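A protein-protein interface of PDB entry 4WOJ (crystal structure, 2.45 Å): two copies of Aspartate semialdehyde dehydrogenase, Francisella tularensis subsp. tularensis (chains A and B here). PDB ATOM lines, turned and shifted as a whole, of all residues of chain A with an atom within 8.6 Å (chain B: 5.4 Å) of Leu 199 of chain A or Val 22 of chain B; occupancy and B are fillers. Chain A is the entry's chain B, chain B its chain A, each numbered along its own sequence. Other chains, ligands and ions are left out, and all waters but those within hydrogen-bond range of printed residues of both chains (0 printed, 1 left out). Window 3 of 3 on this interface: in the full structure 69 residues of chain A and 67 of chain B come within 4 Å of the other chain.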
ATOM      1  N   GLU A 196       5.497  35.998   9.148  1.00  0.00           N
ATOM      2  CA  GLU A 196       6.020  36.120   7.790  1.00  0.00           C
ATOM      3  C   GLU A 196       5.931  34.771   7.034  1.00  0.00           C
ATOM      4  O   GLU A 196       5.872  33.699   7.637  1.00  0.00           O
ATOM      5  CB  GLU A 196       7.440  36.707   7.833  1.00  0.00           C
ATOM      6  CG  GLU A 196       8.039  37.095   6.483  1.00  0.00           C
ATOM      7  CD  GLU A 196       7.180  38.062   5.684  1.00  0.00           C
ATOM      8  OE1 GLU A 196       6.551  37.622   4.679  1.00  0.00           O
ATOM      9  OE2 GLU A 196       7.141  39.253   6.067  1.00  0.00           O
ATOM     10  N   ASP A 197       5.850  34.834   5.714  1.00  0.00           N
ATOM     11  CA  ASP A 197       5.809  33.616   4.883  1.00  0.00           C
ATOM     12  C   ASP A 197       7.077  32.770   5.091  1.00  0.00           C
ATOM     13  O   ASP A 197       8.211  33.291   5.146  1.00  0.00           O
ATOM     14  CB  ASP A 197       5.688  33.984   3.393  1.00  0.00           C
ATOM     15  CG  ASP A 197       4.233  34.284   2.944  1.00  0.00           C
ATOM     16  OD1 ASP A 197       3.264  33.843   3.615  1.00  0.00           O
ATOM     17  OD2 ASP A 197       4.069  34.964   1.898  1.00  0.00           O
ATOM     18  N   ILE A 198       6.885  31.460   5.174  1.00  0.00           N
ATOM     19  CA  ILE A 198       7.983  30.518   5.494  1.00  0.00           C
ATOM     20  C   ILE A 198       9.254  30.648   4.632  1.00  0.00           C
ATOM     21  O   ILE A 198      10.375  30.602   5.173  1.00  0.00           O
ATOM     22  CB  ILE A 198       7.495  29.043   5.492  1.00  0.00           C
ATOM     23  CG1 ILE A 198       8.507  28.130   6.202  1.00  0.00           C
ATOM     24  CG2 ILE A 198       7.187  28.574   4.084  1.00  0.00           C
ATOM     25  CD1 ILE A 198       8.773  28.531   7.642  1.00  0.00           C
ATOM     26  N   LEU A 199       9.104  30.832   3.321  1.00  0.00           N
ATOM     27  CA  LEU A 199      10.306  30.935   2.455  1.00  0.00           C
ATOM     28  C   LEU A 199      10.984  32.276   2.619  1.00  0.00           C
ATOM     29  O   LEU A 199      12.192  32.405   2.442  1.00  0.00           O
ATOM     30  CB  LEU A 199       9.999  30.667   0.982  1.00  0.00           C
ATOM     31  CG  LEU A 199       9.422  29.292   0.652  1.00  0.00           C
ATOM     32  CD1 LEU A 199       9.221  29.139  -0.853  1.00  0.00           C
ATOM     33  CD2 LEU A 199      10.367  28.224   1.156  1.00  0.00           C
ATOM     34  N   ILE A 200      10.211  33.272   3.005  1.00  0.00           N
ATOM     35  CA  ILE A 200      10.777  34.593   3.274  1.00  0.00           C
ATOM     36  C   ILE A 200      11.562  34.582   4.594  1.00  0.00           C
ATOM     37  O   ILE A 200      12.618  35.241   4.738  1.00  0.00           O
ATOM     38  CB  ILE A 200       9.682  35.679   3.177  1.00  0.00           C
ATOM     39  CG1 ILE A 200       9.288  35.817   1.695  1.00  0.00           C
ATOM     40  CG2 ILE A 200      10.140  36.978   3.851  1.00  0.00           C
ATOM     41  CD1 ILE A 200       8.248  36.867   1.389  1.00  0.00           C
ATOM     42  N   ARG A 201      11.064  33.826   5.559  1.00  0.00           N
ATOM     43  CA  ARG A 201      11.778  33.708   6.833  1.00  0.00           C
ATOM     44  C   ARG A 201      13.137  33.079   6.631  1.00  0.00           C
ATOM     45  O   ARG A 201      14.148  33.539   7.163  1.00  0.00           O
ATOM     46  CB  ARG A 201      10.976  32.901   7.829  1.00  0.00           C
ATOM     47  CG  ARG A 201       9.687  33.570   8.306  1.00  0.00           C
ATOM     48  CD  ARG A 201       8.711  32.559   8.911  1.00  0.00           C
ATOM     49  NE  ARG A 201       9.226  32.021  10.138  1.00  0.00           N
ATOM     50  CZ  ARG A 201       8.618  31.110  10.888  1.00  0.00           C
ATOM     51  NH1 ARG A 201       7.467  30.595  10.515  1.00  0.00           N
ATOM     52  NH2 ARG A 201       9.234  30.647  11.988  1.00  0.00           N
ATOM     53  N   GLU A 202      13.144  32.012   5.842  1.00  0.00           N
ATOM     54  CA  GLU A 202      14.361  31.253   5.539  1.00  0.00           C
ATOM     55  C   GLU A 202      15.351  32.229   4.909  1.00  0.00           C
ATOM     56  O   GLU A 202      16.528  32.284   5.298  1.00  0.00           O
ATOM     57  CB  GLU A 202      14.040  30.042   4.637  1.00  0.00           C
ATOM     58  CG  GLU A 202      15.241  29.224   4.187  1.00  0.00           C
ATOM     59  CD  GLU A 202      16.164  30.047   3.289  1.00  0.00           C
ATOM     60  OE1 GLU A 202      17.381  30.164   3.573  1.00  0.00           O
ATOM     61  OE2 GLU A 202      15.631  30.670   2.344  1.00  0.00           O
ATOM     62  N   LYS A 203      14.858  33.017   3.973  1.00  0.00           N
ATOM     63  CA  LYS A 203      15.687  34.014   3.300  1.00  0.00           C
ATOM     64  C   LYS A 203      16.290  35.028   4.241  1.00  0.00           C
ATOM     65  O   LYS A 203      17.493  35.339   4.148  1.00  0.00           O
ATOM     66  CB  LYS A 203      14.851  34.742   2.263  1.00  0.00           C
ATOM     67  CG  LYS A 203      15.657  35.743   1.461  1.00  0.00           C
ATOM     68  CD  LYS A 203      14.805  36.451   0.414  1.00  0.00           C
ATOM     69  CE  LYS A 203      15.473  37.775   0.007  1.00  0.00           C
ATOM     70  NZ  LYS A 203      16.843  37.590  -0.572  1.00  0.00           N
ATOM     71  N   ILE A 204      15.446  35.539   5.152  1.00  0.00           N
ATOM     72  CA  ILE A 204      15.854  36.542   6.139  1.00  0.00           C
ATOM     73  C   ILE A 204      16.939  36.021   7.050  1.00  0.00           C
ATOM     74  O   ILE A 204      17.917  36.717   7.305  1.00  0.00           O
ATOM     75  CB  ILE A 204      14.652  37.046   6.974  1.00  0.00           C
ATOM     76  CG1 ILE A 204      13.827  38.079   6.169  1.00  0.00           C
ATOM     77  CG2 ILE A 204      15.107  37.707   8.263  1.00  0.00           C
ATOM     78  CD1 ILE A 204      12.353  38.124   6.554  1.00  0.00           C
ATOM     79  N   LEU A 205      16.766  34.801   7.547  1.00  0.00           N
ATOM     80  CA  LEU A 205      17.792  34.169   8.400  1.00  0.00           C
ATOM     81  C   LEU A 205      19.056  33.991   7.609  1.00  0.00           C
ATOM     82  O   LEU A 205      20.156  34.337   8.063  1.00  0.00           O
ATOM     83  CB  LEU A 205      17.358  32.790   8.890  1.00  0.00           C
ATOM     84  CG  LEU A 205      16.067  32.664   9.674  1.00  0.00           C
ATOM     85  CD1 LEU A 205      15.852  31.232  10.111  1.00  0.00           C
ATOM     86  CD2 LEU A 205      16.094  33.579  10.875  1.00  0.00           C
ATOM     87  N   ARG A 206      18.880  33.446   6.406  1.00  0.00           N
ATOM     88  CA  ARG A 206      20.012  33.169   5.544  1.00  0.00           C
ATOM     89  C   ARG A 206      20.860  34.420   5.309  1.00  0.00           C
ATOM     90  O   ARG A 206      22.072  34.388   5.516  1.00  0.00           O
ATOM     91  CB  ARG A 206      19.578  32.565   4.219  1.00  0.00           C
ATOM     92  CG  ARG A 206      20.775  32.133   3.388  1.00  0.00           C
ATOM     93  CD  ARG A 206      20.364  31.264   2.225  1.00  0.00           C
ATOM     94  NE  ARG A 206      20.053  32.086   1.055  1.00  0.00           N
ATOM     95  CZ  ARG A 206      18.860  32.190   0.479  1.00  0.00           C
ATOM     96  NH1 ARG A 206      17.825  31.514   0.916  1.00  0.00           N
ATOM     97  NH2 ARG A 206      18.714  32.972  -0.576  1.00  0.00           N
ATOM     98  N   GLY B  17       2.148  24.988  -1.479  1.00  0.00           N
ATOM     99  CA  GLY B  17       3.269  24.588  -0.634  1.00  0.00           C
ATOM    100  C   GLY B  17       4.612  25.075  -1.138  1.00  0.00           C
ATOM    101  O   GLY B  17       4.690  25.931  -2.001  1.00  0.00           O
ATOM    102  N   MET B  18       5.676  24.517  -0.589  1.00  0.00           N
ATOM    103  CA  MET B  18       7.021  25.065  -0.820  1.00  0.00           C
ATOM    104  C   MET B  18       7.553  24.730  -2.206  1.00  0.00           C
ATOM    105  O   MET B  18       8.000  25.616  -2.893  1.00  0.00           O
ATOM    106  CB  MET B  18       8.000  24.578   0.231  1.00  0.00           C
ATOM    107  CG  MET B  18       7.673  25.134   1.580  1.00  0.00           C
ATOM    108  SD  MET B  18       8.829  24.547   2.809  1.00  0.00           S
ATOM    109  CE  MET B  18       9.627  26.064   3.132  1.00  0.00           C
ATOM    110  N   VAL B  19       7.478  23.467  -2.599  1.00  0.00           N
ATOM    111  CA  VAL B  19       7.928  23.059  -3.922  1.00  0.00           C
ATOM    112  C   VAL B  19       7.133  23.872  -4.928  1.00  0.00           C
ATOM    113  O   VAL B  19       7.683  24.464  -5.869  1.00  0.00           O
ATOM    114  CB  VAL B  19       7.698  21.551  -4.183  1.00  0.00           C
ATOM    115  CG1 VAL B  19       8.083  21.172  -5.627  1.00  0.00           C
ATOM    116  CG2 VAL B  19       8.507  20.721  -3.205  1.00  0.00           C
ATOM    117  N   GLY B  20       5.828  23.910  -4.676  1.00  0.00           N
ATOM    118  CA  GLY B  20       4.854  24.604  -5.522  1.00  0.00           C
ATOM    119  C   GLY B  20       5.095  26.081  -5.646  1.00  0.00           C
ATOM    120  O   GLY B  20       4.931  26.624  -6.721  1.00  0.00           O
ATOM    121  N   SER B  21       5.476  26.757  -4.577  1.00  0.00           N
ATOM    122  CA  SER B  21       5.784  28.203  -4.698  1.00  0.00           C
ATOM    123  C   SER B  21       7.098  28.409  -5.437  1.00  0.00           C
ATOM    124  O   SER B  21       7.279  29.360  -6.208  1.00  0.00           O
ATOM    125  CB  SER B  21       5.909  28.897  -3.349  1.00  0.00           C
ATOM    126  OG  SER B  21       5.135  28.212  -2.384  1.00  0.00           O
ATOM    127  N   VAL B  22       8.025  27.520  -5.185  1.00  0.00           N
ATOM    128  CA  VAL B  22       9.293  27.638  -5.845  1.00  0.00           C
ATOM    129  C   VAL B  22       9.100  27.422  -7.347  1.00  0.00           C
ATOM    130  O   VAL B  22       9.731  28.110  -8.159  1.00  0.00           O
ATOM    131  CB  VAL B  22      10.325  26.700  -5.210  1.00  0.00           C
ATOM    132  CG1 VAL B  22      11.610  26.650  -6.037  1.00  0.00           C
ATOM    133  CG2 VAL B  22      10.594  27.244  -3.805  1.00  0.00           C
ATOM    134  N   LEU B  23       8.186  26.514  -7.694  1.00  0.00           N
ATOM    135  CA  LEU B  23       7.863  26.241  -9.095  1.00  0.00           C
ATOM    136  C   LEU B  23       7.209  27.459  -9.720  1.00  0.00           C
ATOM    137  O   LEU B  23       7.617  27.887 -10.789  1.00  0.00           O
ATOM    138  CB  LEU B  23       6.923  25.032  -9.198  1.00  0.00           C
ATOM    139  CG  LEU B  23       6.443  24.695 -10.593  1.00  0.00           C
ATOM    140  CD1 LEU B  23       7.625  24.204 -11.407  1.00  0.00           C
ATOM    141  CD2 LEU B  23       5.326  23.674 -10.581  1.00  0.00           C
ATOM    142  N   MET B  24       6.182  27.987  -9.064  1.00  0.00           N
ATOM    143  CA  MET B  24       5.523  29.202  -9.524  1.00  0.00           C
ATOM    144  C   MET B  24       6.550  30.286  -9.762  1.00  0.00           C
ATOM    145  O   MET B  24       6.623  30.874 -10.814  1.00  0.00           O
ATOM    146  CB  MET B  24       4.512  29.742  -8.490  1.00  0.00           C
ATOM    147  CG  MET B  24       3.294  28.886  -8.291  1.00  0.00           C
ATOM    148  SD  MET B  24       2.514  28.445  -9.863  1.00  0.00           S
ATOM    149  CE  MET B  24       2.937  26.730  -9.949  1.00  0.00           C
ATOM    150  N   SER B  25       7.350  30.563  -8.748  1.00  0.00           N
ATOM    151  CA  SER B  25       8.357  31.609  -8.894  1.00  0.00           C
ATOM    152  C   SER B  25       9.289  31.341 -10.067  1.00  0.00           C
ATOM    153  O   SER B  25       9.750  32.261 -10.708  1.00  0.00           O
ATOM    154  CB  SER B  25       9.204  31.733  -7.652  1.00  0.00           C
ATOM    155  OG  SER B  25      10.406  32.387  -7.994  1.00  0.00           O
ATOM    156  N   ARG B  26       9.595  30.091 -10.327  1.00  0.00           N
ATOM    157  CA  ARG B  26      10.583  29.770 -11.375  1.00  0.00           C
ATOM    158  C   ARG B  26       9.921  29.945 -12.718  1.00  0.00           C
ATOM    159  O   ARG B  26      10.558  30.320 -13.706  1.00  0.00           O
ATOM    160  CB  ARG B  26      11.166  28.364 -11.163  1.00  0.00           C
ATOM    161  CG  ARG B  26      12.248  28.331 -10.092  1.00  0.00           C
ATOM    162  CD  ARG B  26      13.538  29.014 -10.558  1.00  0.00           C
ATOM    163  NE  ARG B  26      14.101  28.359 -11.747  1.00  0.00           N
ATOM    164  CZ  ARG B  26      14.812  28.964 -12.684  1.00  0.00           C
ATOM    165  NH1 ARG B  26      15.081  30.267 -12.568  1.00  0.00           N
ATOM    166  NH2 ARG B  26      15.267  28.270 -13.731  1.00  0.00           N
ATOM    167  N   MET B  27       8.621  29.678 -12.751  1.00  0.00           N
ATOM    168  CA  MET B  27       7.830  29.885 -13.969  1.00  0.00           C
ATOM    169  C   MET B  27       7.634  31.333 -14.294  1.00  0.00           C
ATOM    170  O   MET B  27       7.772  31.721 -15.445  1.00  0.00           O
ATOM    171  CB  MET B  27       6.510  29.107 -13.905  1.00  0.00           C
ATOM    172  CG  MET B  27       6.750  27.594 -14.040  1.00  0.00           C
ATOM    173  SD  MET B  27       5.300  26.553 -13.874  1.00  0.00           S
ATOM    174  CE  MET B  27       4.530  26.759 -15.452  1.00  0.00           C
ATOM    175  N   ARG B 274      16.865  24.409   3.639  1.00  0.00           N
ATOM    176  CA  ARG B 274      16.466  23.986   2.248  1.00  0.00           C
ATOM    177  C   ARG B 274      17.540  23.401   1.352  1.00  0.00           C
ATOM    178  O   ARG B 274      17.272  23.020   0.220  1.00  0.00           O
ATOM    179  CB  ARG B 274      15.765  25.115   1.492  1.00  0.00           C
ATOM    180  CG  ARG B 274      16.293  26.508   1.758  1.00  0.00           C
ATOM    181  CD  ARG B 274      15.585  27.519   0.902  1.00  0.00           C
ATOM    182  NE  ARG B 274      15.443  27.111  -0.484  1.00  0.00           N
ATOM    183  CZ  ARG B 274      14.802  27.840  -1.398  1.00  0.00           C
ATOM    184  NH1 ARG B 274      14.750  27.434  -2.659  1.00  0.00           N
ATOM    185  NH2 ARG B 274      14.235  28.991  -1.053  1.00  0.00           N
ATOM    186  N   LEU B 353      14.538  22.335  -2.846  1.00  0.00           N
ATOM    187  CA  LEU B 353      13.302  22.791  -3.466  1.00  0.00           C
ATOM    188  C   LEU B 353      13.411  22.967  -4.969  1.00  0.00           C
ATOM    189  O   LEU B 353      12.438  22.814  -5.689  1.00  0.00           O
ATOM    190  CB  LEU B 353      12.849  24.078  -2.813  1.00  0.00           C
ATOM    191  CG  LEU B 353      12.405  23.871  -1.359  1.00  0.00           C
ATOM    192  CD1 LEU B 353      12.159  25.181  -0.634  1.00  0.00           C
ATOM    193  CD2 LEU B 353      11.161  23.033  -1.265  1.00  0.00           C
ATOM    194  N   LEU B 354      14.594  23.312  -5.440  1.00  0.00           N
ATOM    195  CA  LEU B 354      14.745  23.684  -6.810  1.00  0.00           C
ATOM    196  C   LEU B 354      15.160  22.444  -7.611  1.00  0.00           C
ATOM    197  O   LEU B 354      14.334  21.719  -8.131  1.00  0.00           O
ATOM    198  CB  LEU B 354      15.809  24.767  -6.908  1.00  0.00           C
ATOM    199  CG  LEU B 354      15.369  26.189  -6.598  1.00  0.00           C
ATOM    200  CD1 LEU B 354      16.549  27.088  -6.339  1.00  0.00           C
ATOM    201  CD2 LEU B 354      14.576  26.756  -7.756  1.00  0.00           C
ATOM    202  N   ALA B 358      11.397  21.169  -7.634  1.00  0.00           N
ATOM    203  CA  ALA B 358      10.640  21.979  -8.610  1.00  0.00           C
ATOM    204  C   ALA B 358      11.212  22.050 -10.000  1.00  0.00           C
ATOM    205  O   ALA B 358      10.490  21.934 -10.987  1.00  0.00           O
ATOM    206  CB  ALA B 358      10.507  23.394  -8.073  1.00  0.00           C
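No position is printed for both chains. Of the 5 pairs that touch across the chains among the printed residues, none has its exchanged pair printed and touching as well.
Of the printed residues of chain B, Leu 199 of chain A touches Met 18, Val 22 and Leu 353. No residue of chain A comes within 4 Å of Gly 20 of chain B. No residue of chain A comes within 4 Å of Ser 21 of chain B. Of the printed residues of chain B, Glu 202 of chain A touches Arg 274. Printed residues of chain A within 4 Å of Leu 353 of chain B: Leu 199 (3.96 Å). Ser 25 of chain B touches none of the printed residues of chain A. Leu 354 of chain B touches none of the printed residues of chain A. The nearest printed residue of chain A that does not touch Leu 353 of chain B is Glu 202 of chain A (7.0 Å).
Hydrophobic or aromatic side chains of chain A that line the printed part of chain B: Ile 198 and Leu 199. Hydrophobic or aromatic side chains of chain B within 4 Å of the printed part of chain A: Met 18, Val 22 and Leu 353. Among the printed residues, no Asp or Glu carboxylate lies within 4 Å of a Lys or Arg side-chain nitrogen of the other chain.
Among the printed residues, merely in contact across the chains: Ile 198 of chain A with Met 18 of chain B, Leu 199 of chain A with Met 18 of chain B, Leu 199 of chain A with Val 22 of chain B, Leu 199 of chain A with Leu 353 of chain B and Glu 202 of chain A with Arg 274 of chain B.
The backbone carbonyl oxygen (O) of Leu 353 of chain B is in hydrogen-bond range of the backbone NH (N) of Ala 358 of chain B (2.8 Å). The side-chain carboxylate (OE2) of Glu 202 of chain A is in salt-bridge range of the guanidinium group (NH1) of Arg 206 of chain A.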
